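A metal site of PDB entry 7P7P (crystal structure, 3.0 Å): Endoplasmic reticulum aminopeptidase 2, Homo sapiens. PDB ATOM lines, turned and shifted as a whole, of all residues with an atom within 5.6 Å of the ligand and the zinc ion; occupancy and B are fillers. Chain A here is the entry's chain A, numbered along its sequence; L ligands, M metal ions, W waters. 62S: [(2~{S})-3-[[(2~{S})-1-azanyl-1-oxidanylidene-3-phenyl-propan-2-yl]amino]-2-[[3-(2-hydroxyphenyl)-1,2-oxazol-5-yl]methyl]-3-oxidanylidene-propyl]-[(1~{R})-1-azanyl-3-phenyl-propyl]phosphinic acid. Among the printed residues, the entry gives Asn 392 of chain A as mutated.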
ATOM      1  N   ASP A 198      34.662 -29.699 -15.872  1.00  0.00           N
ATOM      2  CA  ASP A 198      33.592 -28.840 -16.367  1.00  0.00           C
ATOM      3  C   ASP A 198      34.111 -27.994 -17.521  1.00  0.00           C
ATOM      4  O   ASP A 198      34.996 -27.163 -17.329  1.00  0.00           O
ATOM      5  CB  ASP A 198      33.001 -27.943 -15.280  1.00  0.00           C
ATOM      6  CG  ASP A 198      31.588 -27.501 -15.632  1.00  0.00           C
ATOM      7  OD1 ASP A 198      30.683 -28.332 -15.428  1.00  0.00           O
ATOM      8  OD2 ASP A 198      31.363 -26.379 -16.140  1.00  0.00           O
ATOM      9  N   GLU A 200      31.930 -26.649 -20.514  1.00  0.00           N
ATOM     10  CA  GLU A 200      31.112 -25.664 -21.239  1.00  0.00           C
ATOM     11  C   GLU A 200      31.290 -24.277 -20.657  1.00  0.00           C
ATOM     12  O   GLU A 200      31.249 -24.101 -19.418  1.00  0.00           O
ATOM     13  CB  GLU A 200      29.630 -25.995 -21.231  1.00  0.00           C
ATOM     14  CG  GLU A 200      28.934 -25.399 -22.448  1.00  0.00           C
ATOM     15  CD  GLU A 200      27.425 -25.550 -22.431  1.00  0.00           C
ATOM     16  OE1 GLU A 200      26.921 -26.253 -21.530  1.00  0.00           O
ATOM     17  OE2 GLU A 200      26.729 -25.016 -23.331  1.00  0.00           O
ATOM     18  N   PRO A 201      31.496 -23.250 -21.510  1.00  0.00           N
ATOM     19  CA  PRO A 201      31.518 -23.436 -22.984  1.00  0.00           C
ATOM     20  C   PRO A 201      32.865 -23.705 -23.650  1.00  0.00           C
ATOM     21  O   PRO A 201      32.890 -24.460 -24.622  1.00  0.00           O
ATOM     22  CB  PRO A 201      31.025 -22.097 -23.502  1.00  0.00           C
ATOM     23  CG  PRO A 201      30.765 -21.215 -22.259  1.00  0.00           C
ATOM     24  CD  PRO A 201      31.498 -21.837 -21.136  1.00  0.00           C
ATOM     25  N   ALA A 332      30.308 -24.955  -9.673  1.00  0.00           N
ATOM     26  CA  ALA A 332      29.873 -23.588  -9.964  1.00  0.00           C
ATOM     27  C   ALA A 332      28.504 -23.552 -10.638  1.00  0.00           C
ATOM     28  O   ALA A 332      27.550 -23.025 -10.030  1.00  0.00           O
ATOM     29  CB  ALA A 332      30.935 -22.854 -10.785  1.00  0.00           C
ATOM     30  N   PRO A 333      28.316 -24.076 -11.836  1.00  0.00           N
ATOM     31  CA  PRO A 333      26.960 -24.075 -12.394  1.00  0.00           C
ATOM     32  C   PRO A 333      26.032 -24.926 -11.529  1.00  0.00           C
ATOM     33  O   PRO A 333      26.463 -25.681 -10.662  1.00  0.00           O
ATOM     34  CB  PRO A 333      27.140 -24.660 -13.801  1.00  0.00           C
ATOM     35  CG  PRO A 333      28.380 -25.525 -13.684  1.00  0.00           C
ATOM     36  CD  PRO A 333      29.267 -24.804 -12.695  1.00  0.00           C
ATOM     37  N   GLY A 334      24.735 -24.796 -11.764  1.00  0.00           N
ATOM     38  CA  GLY A 334      23.792 -25.635 -11.051  1.00  0.00           C
ATOM     39  C   GLY A 334      23.902 -27.108 -11.417  1.00  0.00           C
ATOM     40  O   GLY A 334      23.874 -27.973 -10.547  1.00  0.00           O
ATOM     41  N   ALA A 335      24.055 -27.391 -12.714  1.00  0.00           N
ATOM     42  CA  ALA A 335      24.281 -28.745 -13.221  1.00  0.00           C
ATOM     43  C   ALA A 335      24.950 -28.680 -14.585  1.00  0.00           C
ATOM     44  O   ALA A 335      24.939 -27.635 -15.228  1.00  0.00           O
ATOM     45  CB  ALA A 335      22.971 -29.508 -13.309  1.00  0.00           C
ATOM     46  N   MET A 336      25.537 -29.789 -15.063  1.00  0.00           N
ATOM     47  CA  MET A 336      25.956 -29.787 -16.468  1.00  0.00           C
ATOM     48  C   MET A 336      25.690 -31.158 -17.078  1.00  0.00           C
ATOM     49  O   MET A 336      25.956 -32.189 -16.450  1.00  0.00           O
ATOM     50  CB  MET A 336      27.436 -29.388 -16.685  1.00  0.00           C
ATOM     51  CG  MET A 336      27.643 -28.405 -17.883  1.00  0.00           C
ATOM     52  SD  MET A 336      27.821 -28.931 -19.548  1.00  0.00           S
ATOM     53  CE  MET A 336      29.577 -29.336 -19.492  1.00  0.00           C
ATOM     54  N   GLU A 337      25.233 -31.115 -18.322  1.00  0.00           N
ATOM     55  CA  GLU A 337      24.580 -32.102 -19.150  1.00  0.00           C
ATOM     56  C   GLU A 337      25.516 -33.045 -19.896  1.00  0.00           C
ATOM     57  O   GLU A 337      25.084 -33.534 -20.970  1.00  0.00           O
ATOM     58  CB  GLU A 337      23.745 -31.292 -20.161  1.00  0.00           C
ATOM     59  CG  GLU A 337      24.471 -29.955 -20.507  1.00  0.00           C
ATOM     60  CD  GLU A 337      24.048 -29.205 -21.752  1.00  0.00           C
ATOM     61  OE1 GLU A 337      23.810 -29.802 -22.839  1.00  0.00           O
ATOM     62  OE2 GLU A 337      23.940 -27.991 -21.696  1.00  0.00           O
ATOM     63  N   TRP A 363      12.451 -28.158  -6.964  1.00  0.00           N
ATOM     64  CA  TRP A 363      13.652 -27.659  -7.634  1.00  0.00           C
ATOM     65  C   TRP A 363      14.526 -28.818  -8.099  1.00  0.00           C
ATOM     66  O   TRP A 363      15.041 -28.795  -9.229  1.00  0.00           O
ATOM     67  CB  TRP A 363      14.412 -26.679  -6.718  1.00  0.00           C
ATOM     68  CG  TRP A 363      15.904 -26.446  -6.968  1.00  0.00           C
ATOM     69  CD1 TRP A 363      16.945 -27.096  -6.366  1.00  0.00           C
ATOM     70  CD2 TRP A 363      16.502 -25.486  -7.859  1.00  0.00           C
ATOM     71  NE1 TRP A 363      18.146 -26.613  -6.829  1.00  0.00           N
ATOM     72  CE2 TRP A 363      17.910 -25.635  -7.749  1.00  0.00           C
ATOM     73  CE3 TRP A 363      15.993 -24.522  -8.730  1.00  0.00           C
ATOM     74  CZ2 TRP A 363      18.806 -24.858  -8.491  1.00  0.00           C
ATOM     75  CZ3 TRP A 363      16.891 -23.754  -9.475  1.00  0.00           C
ATOM     76  CH2 TRP A 363      18.276 -23.930  -9.356  1.00  0.00           C
ATOM     77  N   ARG A 366      13.269 -30.320 -11.245  1.00  0.00           N
ATOM     78  CA  ARG A 366      13.304 -29.474 -12.436  1.00  0.00           C
ATOM     79  C   ARG A 366      14.670 -29.474 -13.094  1.00  0.00           C
ATOM     80  O   ARG A 366      14.758 -29.458 -14.330  1.00  0.00           O
ATOM     81  CB  ARG A 366      12.929 -28.045 -12.065  1.00  0.00           C
ATOM     82  CG  ARG A 366      11.468 -27.834 -11.703  1.00  0.00           C
ATOM     83  CD  ARG A 366      11.207 -26.361 -11.554  1.00  0.00           C
ATOM     84  NE  ARG A 366      11.812 -25.647 -12.674  1.00  0.00           N
ATOM     85  CZ  ARG A 366      11.866 -24.332 -12.789  1.00  0.00           C
ATOM     86  NH1 ARG A 366      11.373 -23.558 -11.835  1.00  0.00           N
ATOM     87  NH2 ARG A 366      12.456 -23.799 -13.847  1.00  0.00           N
ATOM     88  N   VAL A 367      15.728 -29.484 -12.295  1.00  0.00           N
ATOM     89  CA  VAL A 367      17.070 -29.592 -12.851  1.00  0.00           C
ATOM     90  C   VAL A 367      17.251 -30.926 -13.562  1.00  0.00           C
ATOM     91  O   VAL A 367      17.763 -30.986 -14.692  1.00  0.00           O
ATOM     92  CB  VAL A 367      18.113 -29.419 -11.736  1.00  0.00           C
ATOM     93  CG1 VAL A 367      19.544 -29.371 -12.295  1.00  0.00           C
ATOM     94  CG2 VAL A 367      17.792 -28.220 -10.872  1.00  0.00           C
ATOM     95  N   HIS A 370      15.634 -30.638 -16.685  1.00  0.00           N
ATOM     96  CA  HIS A 370      16.405 -29.812 -17.615  1.00  0.00           C
ATOM     97  C   HIS A 370      17.611 -30.561 -18.159  1.00  0.00           C
ATOM     98  O   HIS A 370      17.839 -30.604 -19.379  1.00  0.00           O
ATOM     99  CB  HIS A 370      16.852 -28.548 -16.892  1.00  0.00           C
ATOM    100  CG  HIS A 370      17.575 -27.540 -17.743  1.00  0.00           C
ATOM    101  ND1 HIS A 370      17.243 -26.210 -17.726  1.00  0.00           N
ATOM    102  CD2 HIS A 370      18.685 -27.638 -18.513  1.00  0.00           C
ATOM    103  CE1 HIS A 370      18.062 -25.536 -18.510  1.00  0.00           C
ATOM    104  NE2 HIS A 370      18.947 -26.378 -19.001  1.00  0.00           N
ATOM    105  N   GLU A 371      18.416 -31.130 -17.268  1.00  0.00           N
ATOM    106  CA  GLU A 371      19.610 -31.805 -17.735  1.00  0.00           C
ATOM    107  C   GLU A 371      19.226 -32.945 -18.695  1.00  0.00           C
ATOM    108  O   GLU A 371      19.836 -33.120 -19.761  1.00  0.00           O
ATOM    109  CB  GLU A 371      20.388 -32.345 -16.533  1.00  0.00           C
ATOM    110  CG  GLU A 371      21.369 -31.380 -15.839  1.00  0.00           C
ATOM    111  CD  GLU A 371      21.878 -30.189 -16.700  1.00  0.00           C
ATOM    112  OE1 GLU A 371      21.352 -29.058 -16.510  1.00  0.00           O
ATOM    113  OE2 GLU A 371      22.735 -30.388 -17.621  1.00  0.00           O
ATOM    114  N   HIS A 374      18.613 -31.991 -22.105  1.00  0.00           N
ATOM    115  CA  HIS A 374      19.793 -31.588 -22.860  1.00  0.00           C
ATOM    116  C   HIS A 374      20.318 -32.752 -23.718  1.00  0.00           C
ATOM    117  O   HIS A 374      20.950 -32.506 -24.764  1.00  0.00           O
ATOM    118  CB  HIS A 374      20.904 -31.082 -21.940  1.00  0.00           C
ATOM    119  CG  HIS A 374      20.833 -29.616 -21.656  1.00  0.00           C
ATOM    120  ND1 HIS A 374      20.653 -28.670 -22.638  1.00  0.00           N
ATOM    121  CD2 HIS A 374      20.971 -28.935 -20.499  1.00  0.00           C
ATOM    122  CE1 HIS A 374      20.643 -27.465 -22.080  1.00  0.00           C
ATOM    123  NE2 HIS A 374      20.830 -27.607 -20.778  1.00  0.00           N
ATOM    124  N   ASN A 392      19.935 -24.531 -27.463  1.00  0.00           N
ATOM    125  CA  ASN A 392      20.081 -25.519 -26.410  1.00  0.00           C
ATOM    126  C   ASN A 392      19.254 -25.103 -25.205  1.00  0.00           C
ATOM    127  O   ASN A 392      18.305 -25.803 -24.828  1.00  0.00           O
ATOM    128  CB  ASN A 392      21.547 -25.660 -25.995  1.00  0.00           C
ATOM    129  CG  ASN A 392      22.365 -26.444 -26.997  1.00  0.00           C
ATOM    130  OD1 ASN A 392      21.879 -26.829 -28.059  1.00  0.00           O
ATOM    131  ND2 ASN A 392      23.607 -26.688 -26.655  1.00  0.00           N
ATOM    132  N   GLU A 393      19.548 -23.922 -24.653  1.00  0.00           N
ATOM    133  CA  GLU A 393      19.098 -23.627 -23.299  1.00  0.00           C
ATOM    134  C   GLU A 393      17.611 -23.290 -23.275  1.00  0.00           C
ATOM    135  O   GLU A 393      16.865 -23.822 -22.442  1.00  0.00           O
ATOM    136  CB  GLU A 393      19.967 -22.518 -22.704  1.00  0.00           C
ATOM    137  CG  GLU A 393      21.458 -22.939 -22.673  1.00  0.00           C
ATOM    138  CD  GLU A 393      21.801 -24.106 -21.727  1.00  0.00           C
ATOM    139  OE1 GLU A 393      23.021 -24.340 -21.488  1.00  0.00           O
ATOM    140  OE2 GLU A 393      20.873 -24.708 -21.137  1.00  0.00           O
ATOM    141  N   ALA A 396      15.753 -26.612 -23.767  1.00  0.00           N
ATOM    142  CA  ALA A 396      15.862 -27.378 -22.531  1.00  0.00           C
ATOM    143  C   ALA A 396      14.966 -26.775 -21.454  1.00  0.00           C
ATOM    144  O   ALA A 396      14.151 -27.480 -20.852  1.00  0.00           O
ATOM    145  CB  ALA A 396      17.305 -27.400 -22.060  1.00  0.00           C
ATOM    146  N   LYS A 397      15.060 -25.446 -21.252  1.00  0.00           N
ATOM    147  CA  LYS A 397      14.230 -24.844 -20.226  1.00  0.00           C
ATOM    148  C   LYS A 397      12.755 -25.053 -20.517  1.00  0.00           C
ATOM    149  O   LYS A 397      11.957 -25.262 -19.590  1.00  0.00           O
ATOM    150  CB  LYS A 397      14.518 -23.362 -20.087  1.00  0.00           C
ATOM    151  CG  LYS A 397      13.388 -22.578 -19.430  1.00  0.00           C
ATOM    152  CD  LYS A 397      13.921 -21.615 -18.339  1.00  0.00           C
ATOM    153  CE  LYS A 397      14.458 -22.384 -17.128  1.00  0.00           C
ATOM    154  NZ  LYS A 397      15.007 -21.510 -16.047  1.00  0.00           N
ATOM    155  N   GLU A 400      11.551 -28.453 -19.371  1.00  0.00           N
ATOM    156  CA  GLU A 400      11.312 -28.614 -17.943  1.00  0.00           C
ATOM    157  C   GLU A 400       9.812 -28.546 -17.698  1.00  0.00           C
ATOM    158  O   GLU A 400       9.225 -29.442 -17.083  1.00  0.00           O
ATOM    159  CB  GLU A 400      12.003 -27.535 -17.087  1.00  0.00           C
ATOM    160  CG  GLU A 400      13.422 -27.133 -17.351  1.00  0.00           C
ATOM    161  CD  GLU A 400      13.880 -26.093 -16.321  1.00  0.00           C
ATOM    162  OE1 GLU A 400      13.002 -25.480 -15.684  1.00  0.00           O
ATOM    163  OE2 GLU A 400      15.094 -25.818 -16.184  1.00  0.00           O
ATOM    164  N   GLN A 447      30.170 -16.474 -22.437  1.00  0.00           N
ATOM    165  CA  GLN A 447      29.619 -16.723 -21.112  1.00  0.00           C
ATOM    166  C   GLN A 447      28.420 -15.820 -20.873  1.00  0.00           C
ATOM    167  O   GLN A 447      27.392 -16.264 -20.352  1.00  0.00           O
ATOM    168  CB  GLN A 447      30.662 -16.554 -20.020  1.00  0.00           C
ATOM    169  CG  GLN A 447      31.310 -17.897 -19.626  1.00  0.00           C
ATOM    170  CD  GLN A 447      32.510 -17.756 -18.687  1.00  0.00           C
ATOM    171  OE1 GLN A 447      33.375 -16.900 -18.887  1.00  0.00           O
ATOM    172  NE2 GLN A 447      32.558 -18.618 -17.652  1.00  0.00           N
ATOM    173  N   PHE A 450      24.590 -16.847 -21.581  1.00  0.00           N
ATOM    174  CA  PHE A 450      23.768 -17.715 -20.721  1.00  0.00           C
ATOM    175  C   PHE A 450      22.982 -16.838 -19.746  1.00  0.00           C
ATOM    176  O   PHE A 450      23.317 -16.692 -18.577  1.00  0.00           O
ATOM    177  CB  PHE A 450      24.640 -18.739 -20.021  1.00  0.00           C
ATOM    178  CG  PHE A 450      25.218 -19.775 -20.960  1.00  0.00           C
ATOM    179  CD1 PHE A 450      24.532 -20.943 -21.239  1.00  0.00           C
ATOM    180  CD2 PHE A 450      26.406 -19.523 -21.638  1.00  0.00           C
ATOM    181  CE1 PHE A 450      25.038 -21.864 -22.129  1.00  0.00           C
ATOM    182  CE2 PHE A 450      26.941 -20.462 -22.525  1.00  0.00           C
ATOM    183  CZ  PHE A 450      26.235 -21.638 -22.782  1.00  0.00           C
ATOM    184  N   TYR A 455      17.523 -18.390 -22.067  1.00  0.00           N
ATOM    185  CA  TYR A 455      16.825 -19.402 -21.279  1.00  0.00           C
ATOM    186  C   TYR A 455      15.335 -19.143 -21.231  1.00  0.00           C
ATOM    187  O   TYR A 455      14.537 -19.945 -21.725  1.00  0.00           O
ATOM    188  CB  TYR A 455      17.317 -19.392 -19.837  1.00  0.00           C
ATOM    189  CG  TYR A 455      18.569 -20.162 -19.677  1.00  0.00           C
ATOM    190  CD1 TYR A 455      19.782 -19.570 -19.978  1.00  0.00           C
ATOM    191  CD2 TYR A 455      18.556 -21.476 -19.225  1.00  0.00           C
ATOM    192  CE1 TYR A 455      20.938 -20.261 -19.809  1.00  0.00           C
ATOM    193  CE2 TYR A 455      19.709 -22.185 -19.068  1.00  0.00           C
ATOM    194  CZ  TYR A 455      20.897 -21.567 -19.363  1.00  0.00           C
ATOM    195  OH  TYR A 455      22.068 -22.249 -19.224  1.00  0.00           O
ATOM    196  N   TYR A 892      28.645 -16.572 -13.914  1.00  0.00           N
ATOM    197  CA  TYR A 892      27.389 -16.181 -13.281  1.00  0.00           C
ATOM    198  C   TYR A 892      27.634 -15.710 -11.869  1.00  0.00           C
ATOM    199  O   TYR A 892      26.835 -14.930 -11.333  1.00  0.00           O
ATOM    200  CB  TYR A 892      26.427 -17.356 -13.321  1.00  0.00           C
ATOM    201  CG  TYR A 892      25.027 -17.096 -12.824  1.00  0.00           C
ATOM    202  CD1 TYR A 892      24.060 -16.475 -13.625  1.00  0.00           C
ATOM    203  CD2 TYR A 892      24.669 -17.532 -11.569  1.00  0.00           C
ATOM    204  CE1 TYR A 892      22.756 -16.294 -13.138  1.00  0.00           C
ATOM    205  CE2 TYR A 892      23.402 -17.357 -11.080  1.00  0.00           C
ATOM    206  CZ  TYR A 892      22.455 -16.741 -11.847  1.00  0.00           C
ATOM    207  OH  TYR A 892      21.232 -16.639 -11.244  1.00  0.00           O
HETATM  208  C15 62S L   1      22.342 -24.207 -15.674  1.00  0.00           C
HETATM  209  C17 62S L   1      19.879 -24.215 -15.399  1.00  0.00           C
HETATM  210  C22 62S L   1      16.966 -24.533 -13.204  1.00  0.00           C
HETATM  211  C24 62S L   1      15.083 -23.608 -12.173  1.00  0.00           C
HETATM  212  C26 62S L   1      15.547 -25.998 -11.955  1.00  0.00           C
HETATM  213  C01 62S L   1      27.401 -23.451 -18.301  1.00  0.00           C
HETATM  214  C02 62S L   1      28.461 -23.661 -17.396  1.00  0.00           C
HETATM  215  C03 62S L   1      29.355 -22.614 -17.151  1.00  0.00           C
HETATM  216  C04 62S L   1      29.199 -21.369 -17.843  1.00  0.00           C
HETATM  217  C05 62S L   1      28.146 -21.184 -18.768  1.00  0.00           C
HETATM  218  C06 62S L   1      27.251 -22.222 -19.011  1.00  0.00           C
HETATM  219  C07 62S L   1      26.500 -24.567 -18.611  1.00  0.00           C
HETATM  220  C08 62S L   1      25.066 -24.725 -18.068  1.00  0.00           C
HETATM  221  C09 62S L   1      24.515 -26.087 -18.467  1.00  0.00           C
HETATM  222  C14 62S L   1      22.645 -25.629 -16.026  1.00  0.00           C
HETATM  223  C16 62S L   1      20.987 -23.793 -16.366  1.00  0.00           C
HETATM  224  C18 62S L   1      18.643 -23.655 -15.042  1.00  0.00           C
HETATM  225  C19 62S L   1      18.200 -24.519 -13.993  1.00  0.00           C
HETATM  226  C23 62S L   1      16.212 -23.438 -12.935  1.00  0.00           C
HETATM  227  C25 62S L   1      14.766 -24.905 -11.694  1.00  0.00           C
HETATM  228  C27 62S L   1      16.657 -25.827 -12.730  1.00  0.00           C
HETATM  229  C29 62S L   1      22.555 -23.564 -14.309  1.00  0.00           C
HETATM  230  C32 62S L   1      21.884 -21.606 -12.753  1.00  0.00           C
HETATM  231  C33 62S L   1      20.605 -21.292 -12.025  1.00  0.00           C
HETATM  232  C36 62S L   1      22.504 -20.309 -13.207  1.00  0.00           C
HETATM  233  C37 62S L   1      23.675 -20.516 -14.193  1.00  0.00           C
HETATM  234  C38 62S L   1      23.448 -20.434 -15.575  1.00  0.00           C
HETATM  235  C39 62S L   1      24.469 -20.676 -16.491  1.00  0.00           C
HETATM  236  C40 62S L   1      25.764 -20.995 -16.064  1.00  0.00           C
HETATM  237  C41 62S L   1      26.015 -21.093 -14.687  1.00  0.00           C
HETATM  238  C42 62S L   1      24.974 -20.859 -13.748  1.00  0.00           C
HETATM  239  N10 62S L   1      24.739 -26.609 -19.807  1.00  0.00           N
HETATM  240  N20 62S L   1      19.119 -25.475 -13.694  1.00  0.00           N
HETATM  241  N31 62S L   1      21.708 -22.390 -13.940  1.00  0.00           N
HETATM  242  N35 62S L   1      20.649 -21.516 -10.573  1.00  0.00           N
HETATM  243  O12 62S L   1      22.001 -27.202 -18.256  1.00  0.00           O
HETATM  244  O13 62S L   1      22.208 -24.917 -19.004  1.00  0.00           O
HETATM  245  O21 62S L   1      20.134 -25.222 -14.564  1.00  0.00           O
HETATM  246  O28 62S L   1      16.564 -22.180 -13.451  1.00  0.00           O
HETATM  247  O30 62S L   1      23.518 -23.915 -13.650  1.00  0.00           O
HETATM  248  O34 62S L   1      19.629 -20.838 -12.639  1.00  0.00           O
HETATM  249  P11 62S L   1      22.754 -25.960 -17.946  1.00  0.00           P
HETATM  250 ZN    ZN M   1      20.655 -25.886 -19.812  1.00  0.00          ZN
HETATM  251  O   HOH W   1      19.727 -19.125  -8.699  1.00  0.00           O
HETATM  252  O   HOH W   2      14.215 -20.658 -11.673  1.00  0.00           O
HETATM  253  O   HOH W   3      16.909 -19.890 -10.994  1.00  0.00           O
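The backbone NH of Gly 334 sits at hydrogen-bond distance from an oxygen (O30) of the ligand, 2.4 Å away. The side-chain carboxylate of Glu 200 is in salt-bridge range of a nitrogen (N10) of the ligand (2.8 Å). The side-chain carboxylate (OE2) of Glu 337 lies within salt-bridge range of a nitrogen (N10) of the ligand, 2.5 Å away. The side-chain hydroxyl (OH) of Tyr 455 lies close to an oxygen (O13) of the ligand (2.7 Å). NZ of Lys 397 sits at hydrogen-bond distance from O28 of the ligand, 3.1 Å away. An oxygen (O12) of the ligand sits close to the side-chain carboxylate (OE1) of Glu 371.
OE1 of Glu 393 sits close to OH of Tyr 455 (3.2 Å). ND1 of His 370 is in hydrogen-bond range of OE2 of Glu 400, 2.7 Å away. NH2 of Arg 366 lies within salt-bridge range of OE1 of Glu 400. OE2 of Glu 371 sits at hydrogen-bond distance from N of Glu 337. A ring nitrogen (ND1) of His 374 sits close to the side-chain carboxylate (OE1) of Glu 337.
Pro 333 touches the ligand. Ala 335 touches the ligand (O to C14, 3.2 Å). SD of Met 336 touches N10 of the ligand (3.9 Å). CE3 of Trp 363 touches C25 of the ligand, at 3.2 Å. Arg 366 touches the ligand. Val 367 touches the ligand. OE2 of Glu 400 touches C22 of the ligand, 3.7 Å away. CG of Phe 450 touches C06 of the ligand, at 3.7 Å. Tyr 892 touches the ligand. Of the 24 residues printed, 18 come within 4 Å of the ligand. Along chain A the residues within 4 Å of the ligand span positions 200 to 892.
Merely in contact with the zinc ion: Tyr 455 (3.9 Å). Of the 24 residues printed, 4 come within 4 Å of the zinc ion.
OE2 of Glu 393 is bound to the zinc ion, at 1.8 Å. NE2 of His 370 binds the zinc ion, at 2.0 Å. A ring nitrogen (NE2) of His 374 binds the zinc ion, 2.0 Å away. An oxygen (O13) of the ligand is bound to the zinc ion, 2.0 Å away. O12 of the ligand is bound to the zinc ion, at 2.4 Å.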
